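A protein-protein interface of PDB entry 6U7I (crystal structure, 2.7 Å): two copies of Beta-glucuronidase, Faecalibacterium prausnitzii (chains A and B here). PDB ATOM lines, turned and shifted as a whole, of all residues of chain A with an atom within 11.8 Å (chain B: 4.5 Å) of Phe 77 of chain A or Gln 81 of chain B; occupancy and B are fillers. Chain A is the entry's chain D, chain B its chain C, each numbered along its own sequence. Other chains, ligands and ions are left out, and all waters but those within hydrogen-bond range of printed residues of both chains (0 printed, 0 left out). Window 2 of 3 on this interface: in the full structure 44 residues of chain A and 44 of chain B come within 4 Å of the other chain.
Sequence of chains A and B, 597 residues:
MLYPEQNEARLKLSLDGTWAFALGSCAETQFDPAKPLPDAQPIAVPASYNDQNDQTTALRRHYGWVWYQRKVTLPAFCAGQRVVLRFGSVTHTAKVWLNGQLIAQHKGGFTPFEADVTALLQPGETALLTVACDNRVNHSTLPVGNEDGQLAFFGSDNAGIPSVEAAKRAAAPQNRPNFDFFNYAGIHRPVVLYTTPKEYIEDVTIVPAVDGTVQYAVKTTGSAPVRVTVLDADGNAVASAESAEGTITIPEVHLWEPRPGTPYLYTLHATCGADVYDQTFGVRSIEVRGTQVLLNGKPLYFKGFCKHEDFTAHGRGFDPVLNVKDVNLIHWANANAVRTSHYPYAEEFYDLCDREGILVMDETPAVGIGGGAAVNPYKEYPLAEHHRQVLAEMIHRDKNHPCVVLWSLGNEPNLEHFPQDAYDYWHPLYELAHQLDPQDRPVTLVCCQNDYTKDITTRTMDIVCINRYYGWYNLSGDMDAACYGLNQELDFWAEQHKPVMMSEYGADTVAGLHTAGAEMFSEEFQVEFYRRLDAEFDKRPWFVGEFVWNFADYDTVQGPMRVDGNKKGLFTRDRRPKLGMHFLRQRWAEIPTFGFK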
ATOM      1  N   GLN A   6      36.874   9.468 -10.089  1.00  0.00           N
ATOM      2  CA  GLN A   6      36.193   9.998  -8.915  1.00  0.00           C
ATOM      3  C   GLN A   6      36.532  11.475  -8.764  1.00  0.00           C
ATOM      4  O   GLN A   6      37.711  11.846  -8.774  1.00  0.00           O
ATOM      5  CB  GLN A   6      36.556   9.218  -7.650  1.00  0.00           C
ATOM      6  CG  GLN A   6      35.991   9.836  -6.379  1.00  0.00           C
ATOM      7  CD  GLN A   6      35.574   8.809  -5.327  1.00  0.00           C
ATOM      8  OE1 GLN A   6      35.049   7.731  -5.640  1.00  0.00           O
ATOM      9  NE2 GLN A   6      35.798   9.153  -4.067  1.00  0.00           N
ATOM     10  N   GLU A   8      34.329  15.612  -7.604  1.00  0.00           N
ATOM     11  CA  GLU A   8      33.143  16.201  -6.989  1.00  0.00           C
ATOM     12  C   GLU A   8      31.866  15.742  -7.670  1.00  0.00           C
ATOM     13  O   GLU A   8      30.780  15.894  -7.090  1.00  0.00           O
ATOM     14  CB  GLU A   8      33.221  17.729  -7.017  1.00  0.00           C
ATOM     15  CG  GLU A   8      33.108  18.341  -8.413  1.00  0.00           C
ATOM     16  CD  GLU A   8      34.457  18.772  -8.989  1.00  0.00           C
ATOM     17  OE1 GLU A   8      35.386  17.926  -9.001  1.00  0.00           O
ATOM     18  OE2 GLU A   8      34.587  19.956  -9.417  1.00  0.00           O
ATOM     19  N   ALA A   9      31.984  15.161  -8.866  1.00  0.00           N
ATOM     20  CA  ALA A   9      30.860  14.761  -9.696  1.00  0.00           C
ATOM     21  C   ALA A   9      30.601  13.263  -9.701  1.00  0.00           C
ATOM     22  O   ALA A   9      29.444  12.834  -9.699  1.00  0.00           O
ATOM     23  CB  ALA A   9      31.090  15.231 -11.131  1.00  0.00           C
ATOM     24  N   ARG A  10      31.641  12.447  -9.743  1.00  0.00           N
ATOM     25  CA  ARG A  10      31.475  11.013  -9.919  1.00  0.00           C
ATOM     26  C   ARG A  10      32.025  10.250  -8.725  1.00  0.00           C
ATOM     27  O   ARG A  10      33.058  10.620  -8.153  1.00  0.00           O
ATOM     28  CB  ARG A  10      32.152  10.546 -11.194  1.00  0.00           C
ATOM     29  CG  ARG A  10      31.830  11.405 -12.416  1.00  0.00           C
ATOM     30  CD  ARG A  10      33.034  11.369 -13.356  1.00  0.00           C
ATOM     31  NE  ARG A  10      32.748  11.761 -14.735  1.00  0.00           N
ATOM     32  CZ  ARG A  10      32.161  10.968 -15.621  1.00  0.00           C
ATOM     33  NH1 ARG A  10      31.773   9.757 -15.261  1.00  0.00           N
ATOM     34  NH2 ARG A  10      31.948  11.386 -16.859  1.00  0.00           N
ATOM     35  N   LEU A  11      31.297   9.206  -8.345  1.00  0.00           N
ATOM     36  CA  LEU A  11      31.700   8.250  -7.331  1.00  0.00           C
ATOM     37  C   LEU A  11      32.221   7.006  -8.040  1.00  0.00           C
ATOM     38  O   LEU A  11      31.749   6.666  -9.127  1.00  0.00           O
ATOM     39  CB  LEU A  11      30.512   7.914  -6.424  1.00  0.00           C
ATOM     40  CG  LEU A  11      30.543   6.796  -5.381  1.00  0.00           C
ATOM     41  CD1 LEU A  11      31.562   7.076  -4.284  1.00  0.00           C
ATOM     42  CD2 LEU A  11      29.152   6.600  -4.780  1.00  0.00           C
ATOM     43  N   LYS A  12      33.235   6.360  -7.446  1.00  0.00           N
ATOM     44  CA  LYS A  12      33.832   5.127  -7.967  1.00  0.00           C
ATOM     45  C   LYS A  12      33.967   4.139  -6.816  1.00  0.00           C
ATOM     46  O   LYS A  12      34.826   4.315  -5.945  1.00  0.00           O
ATOM     47  CB  LYS A  12      35.197   5.392  -8.615  1.00  0.00           C
ATOM     48  CG  LYS A  12      35.969   4.120  -9.092  1.00  0.00           C
ATOM     49  CD  LYS A  12      37.470   4.385  -9.430  1.00  0.00           C
ATOM     50  CE  LYS A  12      38.015   3.434 -10.518  1.00  0.00           C
ATOM     51  NZ  LYS A  12      39.430   2.936 -10.319  1.00  0.00           N
ATOM     52  N   LEU A  13      33.115   3.112  -6.814  1.00  0.00           N
ATOM     53  CA  LEU A  13      33.116   2.040  -5.829  1.00  0.00           C
ATOM     54  C   LEU A  13      33.781   0.790  -6.383  1.00  0.00           C
ATOM     55  O   LEU A  13      33.688   0.488  -7.576  1.00  0.00           O
ATOM     56  CB  LEU A  13      31.690   1.682  -5.407  1.00  0.00           C
ATOM     57  CG  LEU A  13      30.919   2.814  -4.742  1.00  0.00           C
ATOM     58  CD1 LEU A  13      29.607   2.308  -4.116  1.00  0.00           C
ATOM     59  CD2 LEU A  13      31.824   3.485  -3.722  1.00  0.00           C
ATOM     60  N   THR A  73      24.613  -3.364  -2.844  1.00  0.00           N
ATOM     61  CA  THR A  73      23.795  -2.360  -2.179  1.00  0.00           C
ATOM     62  C   THR A  73      24.346  -0.980  -2.492  1.00  0.00           C
ATOM     63  O   THR A  73      25.525  -0.702  -2.231  1.00  0.00           O
ATOM     64  CB  THR A  73      23.778  -2.570  -0.666  1.00  0.00           C
ATOM     65  OG1 THR A  73      23.720  -3.972  -0.388  1.00  0.00           O
ATOM     66  CG2 THR A  73      22.601  -1.851   0.000  1.00  0.00           C
ATOM     67  N   LEU A  74      23.488  -0.120  -3.040  1.00  0.00           N
ATOM     68  CA  LEU A  74      23.793   1.288  -3.212  1.00  0.00           C
ATOM     69  C   LEU A  74      23.143   2.056  -2.082  1.00  0.00           C
ATOM     70  O   LEU A  74      21.913   2.000  -1.955  1.00  0.00           O
ATOM     71  CB  LEU A  74      23.269   1.784  -4.551  1.00  0.00           C
ATOM     72  CG  LEU A  74      23.522   3.261  -4.818  1.00  0.00           C
ATOM     73  CD1 LEU A  74      25.013   3.505  -5.048  1.00  0.00           C
ATOM     74  CD2 LEU A  74      22.664   3.747  -5.999  1.00  0.00           C
ATOM     75  N   PRO A  75      23.898   2.773  -1.249  1.00  0.00           N
ATOM     76  CA  PRO A  75      23.314   3.347  -0.030  1.00  0.00           C
ATOM     77  C   PRO A  75      22.188   4.316  -0.357  1.00  0.00           C
ATOM     78  O   PRO A  75      22.078   4.833  -1.471  1.00  0.00           O
ATOM     79  CB  PRO A  75      24.492   4.071   0.640  1.00  0.00           C
ATOM     80  CG  PRO A  75      25.692   3.762  -0.159  1.00  0.00           C
ATOM     81  CD  PRO A  75      25.249   3.294  -1.506  1.00  0.00           C
ATOM     82  N   ALA A  76      21.340   4.550   0.645  1.00  0.00           N
ATOM     83  CA  ALA A  76      20.197   5.433   0.453  1.00  0.00           C
ATOM     84  C   ALA A  76      20.641   6.860   0.148  1.00  0.00           C
ATOM     85  O   ALA A  76      20.052   7.528  -0.704  1.00  0.00           O
ATOM     86  CB  ALA A  76      19.287   5.389   1.681  1.00  0.00           C
ATOM     87  N   PHE A  77      21.700   7.335   0.784  1.00  0.00           N
ATOM     88  CA  PHE A  77      22.068   8.732   0.581  1.00  0.00           C
ATOM     89  C   PHE A  77      22.788   9.003  -0.743  1.00  0.00           C
ATOM     90  O   PHE A  77      23.058  10.176  -1.036  1.00  0.00           O
ATOM     91  CB  PHE A  77      22.946   9.203   1.730  1.00  0.00           C
ATOM     92  CG  PHE A  77      24.306   8.599   1.720  1.00  0.00           C
ATOM     93  CD1 PHE A  77      25.376   9.266   1.128  1.00  0.00           C
ATOM     94  CD2 PHE A  77      24.527   7.362   2.300  1.00  0.00           C
ATOM     95  CE1 PHE A  77      26.643   8.712   1.116  1.00  0.00           C
ATOM     96  CE2 PHE A  77      25.799   6.797   2.299  1.00  0.00           C
ATOM     97  CZ  PHE A  77      26.853   7.474   1.708  1.00  0.00           C
ATOM     98  N   CYS A  78      23.129   7.971  -1.531  1.00  0.00           N
ATOM     99  CA  CYS A  78      23.852   8.153  -2.801  1.00  0.00           C
ATOM    100  C   CYS A  78      22.837   8.281  -3.929  1.00  0.00           C
ATOM    101  O   CYS A  78      22.656   7.393  -4.768  1.00  0.00           O
ATOM    102  CB  CYS A  78      24.823   7.003  -3.050  1.00  0.00           C
ATOM    103  SG  CYS A  78      26.289   6.904  -1.940  1.00  0.00           S
ATOM    104  N   ALA A  79      22.153   9.419  -3.954  1.00  0.00           N
ATOM    105  CA  ALA A  79      20.900   9.488  -4.686  1.00  0.00           C
ATOM    106  C   ALA A  79      20.975  10.342  -5.953  1.00  0.00           C
ATOM    107  O   ALA A  79      21.832  11.224  -6.114  1.00  0.00           O
ATOM    108  CB  ALA A  79      19.796  10.002  -3.765  1.00  0.00           C
ATOM    109  N   GLY A  80      20.039  10.055  -6.858  1.00  0.00           N
ATOM    110  CA  GLY A  80      19.799  10.903  -8.016  1.00  0.00           C
ATOM    111  C   GLY A  80      20.918  10.984  -9.027  1.00  0.00           C
ATOM    112  O   GLY A  80      21.082  12.023  -9.678  1.00  0.00           O
ATOM    113  N   GLN A  81      21.698   9.912  -9.181  1.00  0.00           N
ATOM    114  CA  GLN A  81      22.774   9.873 -10.156  1.00  0.00           C
ATOM    115  C   GLN A  81      22.595   8.692 -11.106  1.00  0.00           C
ATOM    116  O   GLN A  81      21.874   7.727 -10.819  1.00  0.00           O
ATOM    117  CB  GLN A  81      24.137   9.797  -9.462  1.00  0.00           C
ATOM    118  CG  GLN A  81      24.291  10.736  -8.293  1.00  0.00           C
ATOM    119  CD  GLN A  81      24.310  12.203  -8.698  1.00  0.00           C
ATOM    120  OE1 GLN A  81      25.144  12.635  -9.493  1.00  0.00           O
ATOM    121  NE2 GLN A  81      23.385  12.983  -8.132  1.00  0.00           N
ATOM    122  N   ARG A  82      23.248   8.793 -12.262  1.00  0.00           N
ATOM    123  CA  ARG A  82      23.367   7.663 -13.178  1.00  0.00           C
ATOM    124  C   ARG A  82      24.432   6.696 -12.663  1.00  0.00           C
ATOM    125  O   ARG A  82      25.600   7.070 -12.535  1.00  0.00           O
ATOM    126  CB  ARG A  82      23.730   8.160 -14.576  1.00  0.00           C
ATOM    127  CG  ARG A  82      23.877   7.061 -15.623  1.00  0.00           C
ATOM    128  CD  ARG A  82      24.967   7.392 -16.632  1.00  0.00           C
ATOM    129  NE  ARG A  82      24.976   6.461 -17.763  1.00  0.00           N
ATOM    130  CZ  ARG A  82      26.064   6.060 -18.426  1.00  0.00           C
ATOM    131  NH1 ARG A  82      27.285   6.492 -18.089  1.00  0.00           N
ATOM    132  NH2 ARG A  82      25.925   5.208 -19.434  1.00  0.00           N
ATOM    133  N   VAL A  83      24.037   5.454 -12.384  1.00  0.00           N
ATOM    134  CA  VAL A  83      24.909   4.432 -11.816  1.00  0.00           C
ATOM    135  C   VAL A  83      25.238   3.386 -12.882  1.00  0.00           C
ATOM    136  O   VAL A  83      24.347   2.709 -13.401  1.00  0.00           O
ATOM    137  CB  VAL A  83      24.268   3.775 -10.586  1.00  0.00           C
ATOM    138  CG1 VAL A  83      25.287   2.887  -9.860  1.00  0.00           C
ATOM    139  CG2 VAL A  83      23.748   4.840  -9.637  1.00  0.00           C
ATOM    140  N   LEU A 121      19.109  -0.461  -9.913  1.00  0.00           N
ATOM    141  CA  LEU A 121      19.752  -0.350  -8.610  1.00  0.00           C
ATOM    142  C   LEU A 121      19.389   1.029  -8.041  1.00  0.00           C
ATOM    143  O   LEU A 121      20.101   2.021  -8.227  1.00  0.00           O
ATOM    144  CB  LEU A 121      21.268  -0.567  -8.725  1.00  0.00           C
ATOM    145  CG  LEU A 121      21.983  -0.934  -7.421  1.00  0.00           C
ATOM    146  CD1 LEU A 121      21.395  -2.189  -6.778  1.00  0.00           C
ATOM    147  CD2 LEU A 121      23.464  -1.091  -7.664  1.00  0.00           C
ATOM    148  N   GLN A 122      18.248   1.087  -7.364  1.00  0.00           N
ATOM    149  CA  GLN A 122      17.795   2.313  -6.732  1.00  0.00           C
ATOM    150  C   GLN A 122      18.621   2.560  -5.488  1.00  0.00           C
ATOM    151  O   GLN A 122      19.224   1.633  -4.942  1.00  0.00           O
ATOM    152  CB  GLN A 122      16.324   2.210  -6.346  1.00  0.00           C
ATOM    153  CG  GLN A 122      15.406   2.023  -7.519  1.00  0.00           C
ATOM    154  CD  GLN A 122      15.679   3.041  -8.603  1.00  0.00           C
ATOM    155  OE1 GLN A 122      16.443   2.775  -9.532  1.00  0.00           O
ATOM    156  NE2 GLN A 122      15.063   4.219  -8.490  1.00  0.00           N
ATOM    157  N   PRO A 123      18.682   3.798  -5.022  1.00  0.00           N
ATOM    158  CA  PRO A 123      19.342   4.036  -3.738  1.00  0.00           C
ATOM    159  C   PRO A 123      18.622   3.296  -2.614  1.00  0.00           C
ATOM    160  O   PRO A 123      17.399   3.346  -2.492  1.00  0.00           O
ATOM    161  CB  PRO A 123      19.278   5.557  -3.588  1.00  0.00           C
ATOM    162  CG  PRO A 123      19.333   6.037  -5.014  1.00  0.00           C
ATOM    163  CD  PRO A 123      18.504   5.040  -5.791  1.00  0.00           C
ATOM    164  N   GLY A 124      19.396   2.554  -1.827  1.00  0.00           N
ATOM    165  CA  GLY A 124      18.917   1.931  -0.613  1.00  0.00           C
ATOM    166  C   GLY A 124      18.733   0.435  -0.691  1.00  0.00           C
ATOM    167  O   GLY A 124      18.643  -0.213   0.360  1.00  0.00           O
ATOM    168  N   GLU A 125      18.688  -0.142  -1.888  1.00  0.00           N
ATOM    169  CA  GLU A 125      18.362  -1.554  -2.053  1.00  0.00           C
ATOM    170  C   GLU A 125      19.604  -2.364  -2.423  1.00  0.00           C
ATOM    171  O   GLU A 125      20.694  -1.823  -2.652  1.00  0.00           O
ATOM    172  CB  GLU A 125      17.288  -1.725  -3.122  1.00  0.00           C
ATOM    173  CG  GLU A 125      17.675  -1.015  -4.398  1.00  0.00           C
ATOM    174  CD  GLU A 125      16.699  -1.247  -5.525  1.00  0.00           C
ATOM    175  OE1 GLU A 125      17.175  -1.639  -6.623  1.00  0.00           O
ATOM    176  OE2 GLU A 125      15.470  -1.012  -5.316  1.00  0.00           O
ATOM    177  N   THR A 126      19.405  -3.684  -2.509  1.00  0.00           N
ATOM    178  CA  THR A 126      20.466  -4.660  -2.750  1.00  0.00           C
ATOM    179  C   THR A 126      20.060  -5.618  -3.860  1.00  0.00           C
ATOM    180  O   THR A 126      19.121  -6.404  -3.694  1.00  0.00           O
ATOM    181  CB  THR A 126      20.788  -5.474  -1.488  1.00  0.00           C
ATOM    182  OG1 THR A 126      21.088  -4.605  -0.393  1.00  0.00           O
ATOM    183  CG2 THR A 126      21.980  -6.367  -1.757  1.00  0.00           C
ATOM    184  N   THR A 195      29.290   6.411 -10.811  1.00  0.00           N
ATOM    185  CA  THR A 195      28.162   7.309 -11.022  1.00  0.00           C
ATOM    186  C   THR A 195      28.540   8.464 -11.938  1.00  0.00           C
ATOM    187  O   THR A 195      29.709   8.848 -12.040  1.00  0.00           O
ATOM    188  CB  THR A 195      27.621   7.901  -9.708  1.00  0.00           C
ATOM    189  OG1 THR A 195      28.573   8.839  -9.185  1.00  0.00           O
ATOM    190  CG2 THR A 195      27.330   6.802  -8.679  1.00  0.00           C
ATOM    191  N   GLU B   8      22.418   0.039   3.032  1.00  0.00           N
ATOM    192  CA  GLU B   8      21.584   1.191   2.709  1.00  0.00           C
ATOM    193  C   GLU B   8      21.989   2.439   3.491  1.00  0.00           C
ATOM    194  O   GLU B   8      21.607   3.552   3.108  1.00  0.00           O
ATOM    195  CB  GLU B   8      20.113   0.859   2.968  1.00  0.00           C
ATOM    196  CG  GLU B   8      19.812   0.287   4.357  1.00  0.00           C
ATOM    197  CD  GLU B   8      19.933  -1.241   4.413  1.00  0.00           C
ATOM    198  OE1 GLU B   8      20.862  -1.805   3.767  1.00  0.00           O
ATOM    199  OE2 GLU B   8      19.101  -1.877   5.110  1.00  0.00           O
ATOM    200  N   ALA B   9      22.770   2.280   4.561  1.00  0.00           N
ATOM    201  CA  ALA B   9      23.212   3.403   5.370  1.00  0.00           C
ATOM    202  C   ALA B   9      24.675   3.779   5.168  1.00  0.00           C
ATOM    203  O   ALA B   9      25.048   4.926   5.452  1.00  0.00           O
ATOM    204  CB  ALA B   9      22.978   3.101   6.861  1.00  0.00           C
ATOM    205  N   LEU B  11      28.482   3.689   3.013  1.00  0.00           N
ATOM    206  CA  LEU B  11      29.283   3.589   1.800  1.00  0.00           C
ATOM    207  C   LEU B  11      30.686   3.069   2.136  1.00  0.00           C
ATOM    208  O   LEU B  11      31.289   3.482   3.130  1.00  0.00           O
ATOM    209  CB  LEU B  11      29.357   4.964   1.122  1.00  0.00           C
ATOM    210  CG  LEU B  11      30.109   5.151  -0.199  1.00  0.00           C
ATOM    211  CD1 LEU B  11      29.498   4.251  -1.251  1.00  0.00           C
ATOM    212  CD2 LEU B  11      30.096   6.620  -0.636  1.00  0.00           C
ATOM    213  N   PHE B  77      27.398  14.984  -3.904  1.00  0.00           N
ATOM    214  CA  PHE B  77      26.065  14.475  -3.599  1.00  0.00           C
ATOM    215  C   PHE B  77      26.067  13.431  -2.487  1.00  0.00           C
ATOM    216  O   PHE B  77      24.990  13.000  -2.058  1.00  0.00           O
ATOM    217  CB  PHE B  77      25.416  13.888  -4.862  1.00  0.00           C
ATOM    218  CG  PHE B  77      26.024  12.594  -5.307  1.00  0.00           C
ATOM    219  CD1 PHE B  77      25.427  11.382  -4.976  1.00  0.00           C
ATOM    220  CD2 PHE B  77      27.193  12.587  -6.045  1.00  0.00           C
ATOM    221  CE1 PHE B  77      25.986  10.183  -5.369  1.00  0.00           C
ATOM    222  CE2 PHE B  77      27.761  11.398  -6.441  1.00  0.00           C
ATOM    223  CZ  PHE B  77      27.158  10.192  -6.101  1.00  0.00           C
ATOM    224  N   CYS B  78      27.246  13.010  -2.025  1.00  0.00           N
ATOM    225  CA  CYS B  78      27.363  12.100  -0.891  1.00  0.00           C
ATOM    226  C   CYS B  78      27.213  12.935   0.385  1.00  0.00           C
ATOM    227  O   CYS B  78      28.159  13.183   1.143  1.00  0.00           O
ATOM    228  CB  CYS B  78      28.668  11.320  -0.973  1.00  0.00           C
ATOM    229  SG  CYS B  78      28.849  10.431  -2.583  1.00  0.00           S
ATOM    230  N   ALA B  79      25.961  13.353   0.622  1.00  0.00           N
ATOM    231  CA  ALA B  79      25.659  14.520   1.447  1.00  0.00           C
ATOM    232  C   ALA B  79      25.459  14.158   2.907  1.00  0.00           C
ATOM    233  O   ALA B  79      24.858  13.131   3.238  1.00  0.00           O
ATOM    234  CB  ALA B  79      24.414  15.235   0.919  1.00  0.00           C
ATOM    235  N   GLY B  80      25.951  15.030   3.775  1.00  0.00           N
ATOM    236  CA  GLY B  80      25.724  14.898   5.198  1.00  0.00           C
ATOM    237  C   GLY B  80      25.834  13.527   5.842  1.00  0.00           C
ATOM    238  O   GLY B  80      24.973  13.135   6.642  1.00  0.00           O
ATOM    239  N   GLN B  81      26.880  12.780   5.522  1.00  0.00           N
ATOM    240  CA  GLN B  81      27.155  11.575   6.282  1.00  0.00           C
ATOM    241  C   GLN B  81      28.324  11.841   7.224  1.00  0.00           C
ATOM    242  O   GLN B  81      28.938  12.913   7.211  1.00  0.00           O
ATOM    243  CB  GLN B  81      27.434  10.394   5.355  1.00  0.00           C
ATOM    244  CG  GLN B  81      26.301  10.088   4.388  1.00  0.00           C
ATOM    245  CD  GLN B  81      24.943   9.813   5.065  1.00  0.00           C
ATOM    246  OE1 GLN B  81      24.849   9.048   6.030  1.00  0.00           O
ATOM    247  NE2 GLN B  81      23.885  10.420   4.530  1.00  0.00           N
ATOM    248  N   ARG B  82      28.616  10.861   8.067  1.00  0.00           N
ATOM    249  CA  ARG B  82      29.809  10.897   8.900  1.00  0.00           C
ATOM    250  C   ARG B  82      30.896  10.048   8.237  1.00  0.00           C
ATOM    251  O   ARG B  82      30.711   8.844   8.037  1.00  0.00           O
ATOM    252  CB  ARG B  82      29.476  10.402  10.300  1.00  0.00           C
ATOM    253  CG  ARG B  82      30.629  10.389  11.238  1.00  0.00           C
ATOM    254  CD  ARG B  82      30.991   8.974  11.506  1.00  0.00           C
ATOM    255  NE  ARG B  82      31.796   8.835  12.705  1.00  0.00           N
ATOM    256  CZ  ARG B  82      32.261   7.670  13.127  1.00  0.00           C
ATOM    257  NH1 ARG B  82      31.983   6.568  12.425  1.00  0.00           N
ATOM    258  NH2 ARG B  82      32.981   7.614  14.244  1.00  0.00           N
ATOM    259  N   VAL B  83      32.020  10.681   7.896  1.00  0.00           N
ATOM    260  CA  VAL B  83      33.046  10.102   7.025  1.00  0.00           C
ATOM    261  C   VAL B  83      34.244   9.700   7.872  1.00  0.00           C
ATOM    262  O   VAL B  83      34.720  10.495   8.702  1.00  0.00           O
ATOM    263  CB  VAL B  83      33.460  11.102   5.930  1.00  0.00           C
ATOM    264  CG1 VAL B  83      34.471  10.503   4.998  1.00  0.00           C
ATOM    265  CG2 VAL B  83      32.238  11.561   5.154  1.00  0.00           C
ATOM    266  N   THR B 118      35.090  13.845   9.208  1.00  0.00           N
ATOM    267  CA  THR B 118      33.906  14.511   8.662  1.00  0.00           C
ATOM    268  C   THR B 118      34.101  16.018   8.588  1.00  0.00           C
ATOM    269  O   THR B 118      33.604  16.674   7.664  1.00  0.00           O
ATOM    270  CB  THR B 118      32.664  14.199   9.496  1.00  0.00           C
ATOM    271  OG1 THR B 118      32.673  12.834   9.912  1.00  0.00           O
ATOM    272  CG2 THR B 118      31.410  14.434   8.683  1.00  0.00           C
ATOM    273  N   THR B 195      31.406   5.824   5.437  1.00  0.00           N
ATOM    274  CA  THR B 195      30.359   6.699   5.931  1.00  0.00           C
ATOM    275  C   THR B 195      29.455   5.894   6.853  1.00  0.00           C
ATOM    276  O   THR B 195      29.177   4.714   6.589  1.00  0.00           O
ATOM    277  CB  THR B 195      29.507   7.258   4.780  1.00  0.00           C
ATOM    278  OG1 THR B 195      28.965   6.159   4.054  1.00  0.00           O
ATOM    279  CG2 THR B 195      30.304   8.163   3.826  1.00  0.00           C
ATOM    280  N   THR B 196      29.001   6.533   7.929  1.00  0.00           N
ATOM    281  CA  THR B 196      27.860   6.098   8.721  1.00  0.00           C
ATOM    282  C   THR B 196      26.904   7.259   8.943  1.00  0.00           C
ATOM    283  O   THR B 196      27.247   8.420   8.692  1.00  0.00           O
ATOM    284  CB  THR B 196      28.320   5.525  10.068  1.00  0.00           C
ATOM    285  OG1 THR B 196      28.796   6.591  10.908  1.00  0.00           O
ATOM    286  CG2 THR B 196      29.395   4.451   9.873  1.00  0.00           C
ATOM    287  N   PRO B 197      25.676   6.981   9.395  1.00  0.00           N
ATOM    288  CA  PRO B 197      24.768   8.075   9.765  1.00  0.00           C
ATOM    289  C   PRO B 197      25.391   8.957  10.838  1.00  0.00           C
ATOM    290  O   PRO B 197      26.370   8.578  11.491  1.00  0.00           O
ATOM    291  CB  PRO B 197      23.521   7.345  10.286  1.00  0.00           C
ATOM    292  CG  PRO B 197      23.473   6.111   9.490  1.00  0.00           C
ATOM    293  CD  PRO B 197      24.952   5.702   9.285  1.00  0.00           C
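The backbone NH (N) of Ala 76 of chain A lies within hydrogen-bond range of the backbone carbonyl oxygen (O) of Glu 8 of chain B, 2.7 Å away.
The side-chain hydroxyl of Thr 73 of chain A is in hydrogen-bond range of the side-chain hydroxyl of Thr 126 of chain A (2.7 Å).
The backbone NH of Gly 124 of chain A lies within hydrogen-bond range of the backbone carbonyl oxygen of Leu 74 of chain A (2.6 Å).
The backbone carbonyl oxygen (O) of Ala 79 of chain A is in hydrogen-bond range of the side-chain amide nitrogen (NE2) of Gln 81 of chain A (3.1 Å).
Phe 77 of chain B touches Ala 9 of chain A (CE2 to O, 3.9 Å).
CD1 of Leu 11 of chain B touches CD1 of Leu 13 of chain A (3.5 Å).
Pro 75 of chain A touches Glu 8 of chain B.
Phe 77 of chain A touches Phe 77 of chain B (O to O, 3.6 Å).
CB of Cys 78 of chain B touches CE1 of Phe 77 of chain A, 3.9 Å away.
Thr 195 of chain B touches Phe 77 of chain A.
Gly 124 of chain A touches Glu 8 of chain B.
Thr 195 of chain A touches Phe 77 of chain B (OG1 to CZ, 3.7 Å).
Printed residues of chain B within 4 Å of Thr 73 of chain A: Glu 8.
Of chain B, only Ala 9 (3.7 Å), Leu 11 (3.6 Å), Phe 77 (3.6 Å), Cys 78 (3.9 Å), Gln 81 (3.2 Å) and Thr 195 (3.4 Å) come within 4 Å of Phe 77 of chain A.
Arg 82 of chain A touches none of the printed residues of chain B.
Of the printed residues of chain B, Gly 124 of chain A touches Glu 8.
Of the printed residues of chain A, Leu 11 of chain B touches Leu 11 (3.96 Å), Leu 13 (3.5 Å), Pro 75 (3.99 Å) and Phe 77 (3.6 Å).
No residue of chain A comes within 4 Å of Ala 79 of chain B.
Of the printed residues of chain A, Gln 81 of chain B touches Phe 77 (3.2 Å).
Arg 82 of chain B touches none of the printed residues of chain A.
Thr 195 of chain B touches just one residue of chain A: Phe 77 (3.4 Å).
No residue of chain A comes within 4 Å of Pro 197 of chain B.
The nearest residue of chain A that does not touch Gln 81 of chain B is Ala 76 of chain A (6.5 Å).
The nearest printed residue of chain B that does not touch Leu 11 of chain A is Phe 77 of chain B (4.1 Å).
Of the 14 printed residues of chain B, 7 touch a printed residue of chain A.
Printed residues of chain B that touch a printed residue of chain A: Glu 8, Ala 9, Leu 11, Phe 77, Cys 78, Gln 81 and Thr 195.
Hydrophobic or aromatic side chains of chain B that line the printed part of chain A: Leu 11 and Phe 77.
Among the printed residues, 18 pairs touch across the chains.
Among the printed residues, no Asp or Glu carboxylate lies within 4 Å of a Lys or Arg side-chain nitrogen of the other chain.
Ala 9 of chain A touches Phe 77 of chain B, and with the chains exchanged Phe 77 of chain A touches Ala 9 of chain B.
Phe 77 of chain B touches its own counterpart, Phe 77 of chain A.
Phe 77 of chain A touches Cys 78 of chain B, and with the chains exchanged Cys 78 of chain A touches Phe 77 of chain B.
Of the 18 pairs that touch across the chains among the printed residues, 10 have their exchanged pair printed and touching as well.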
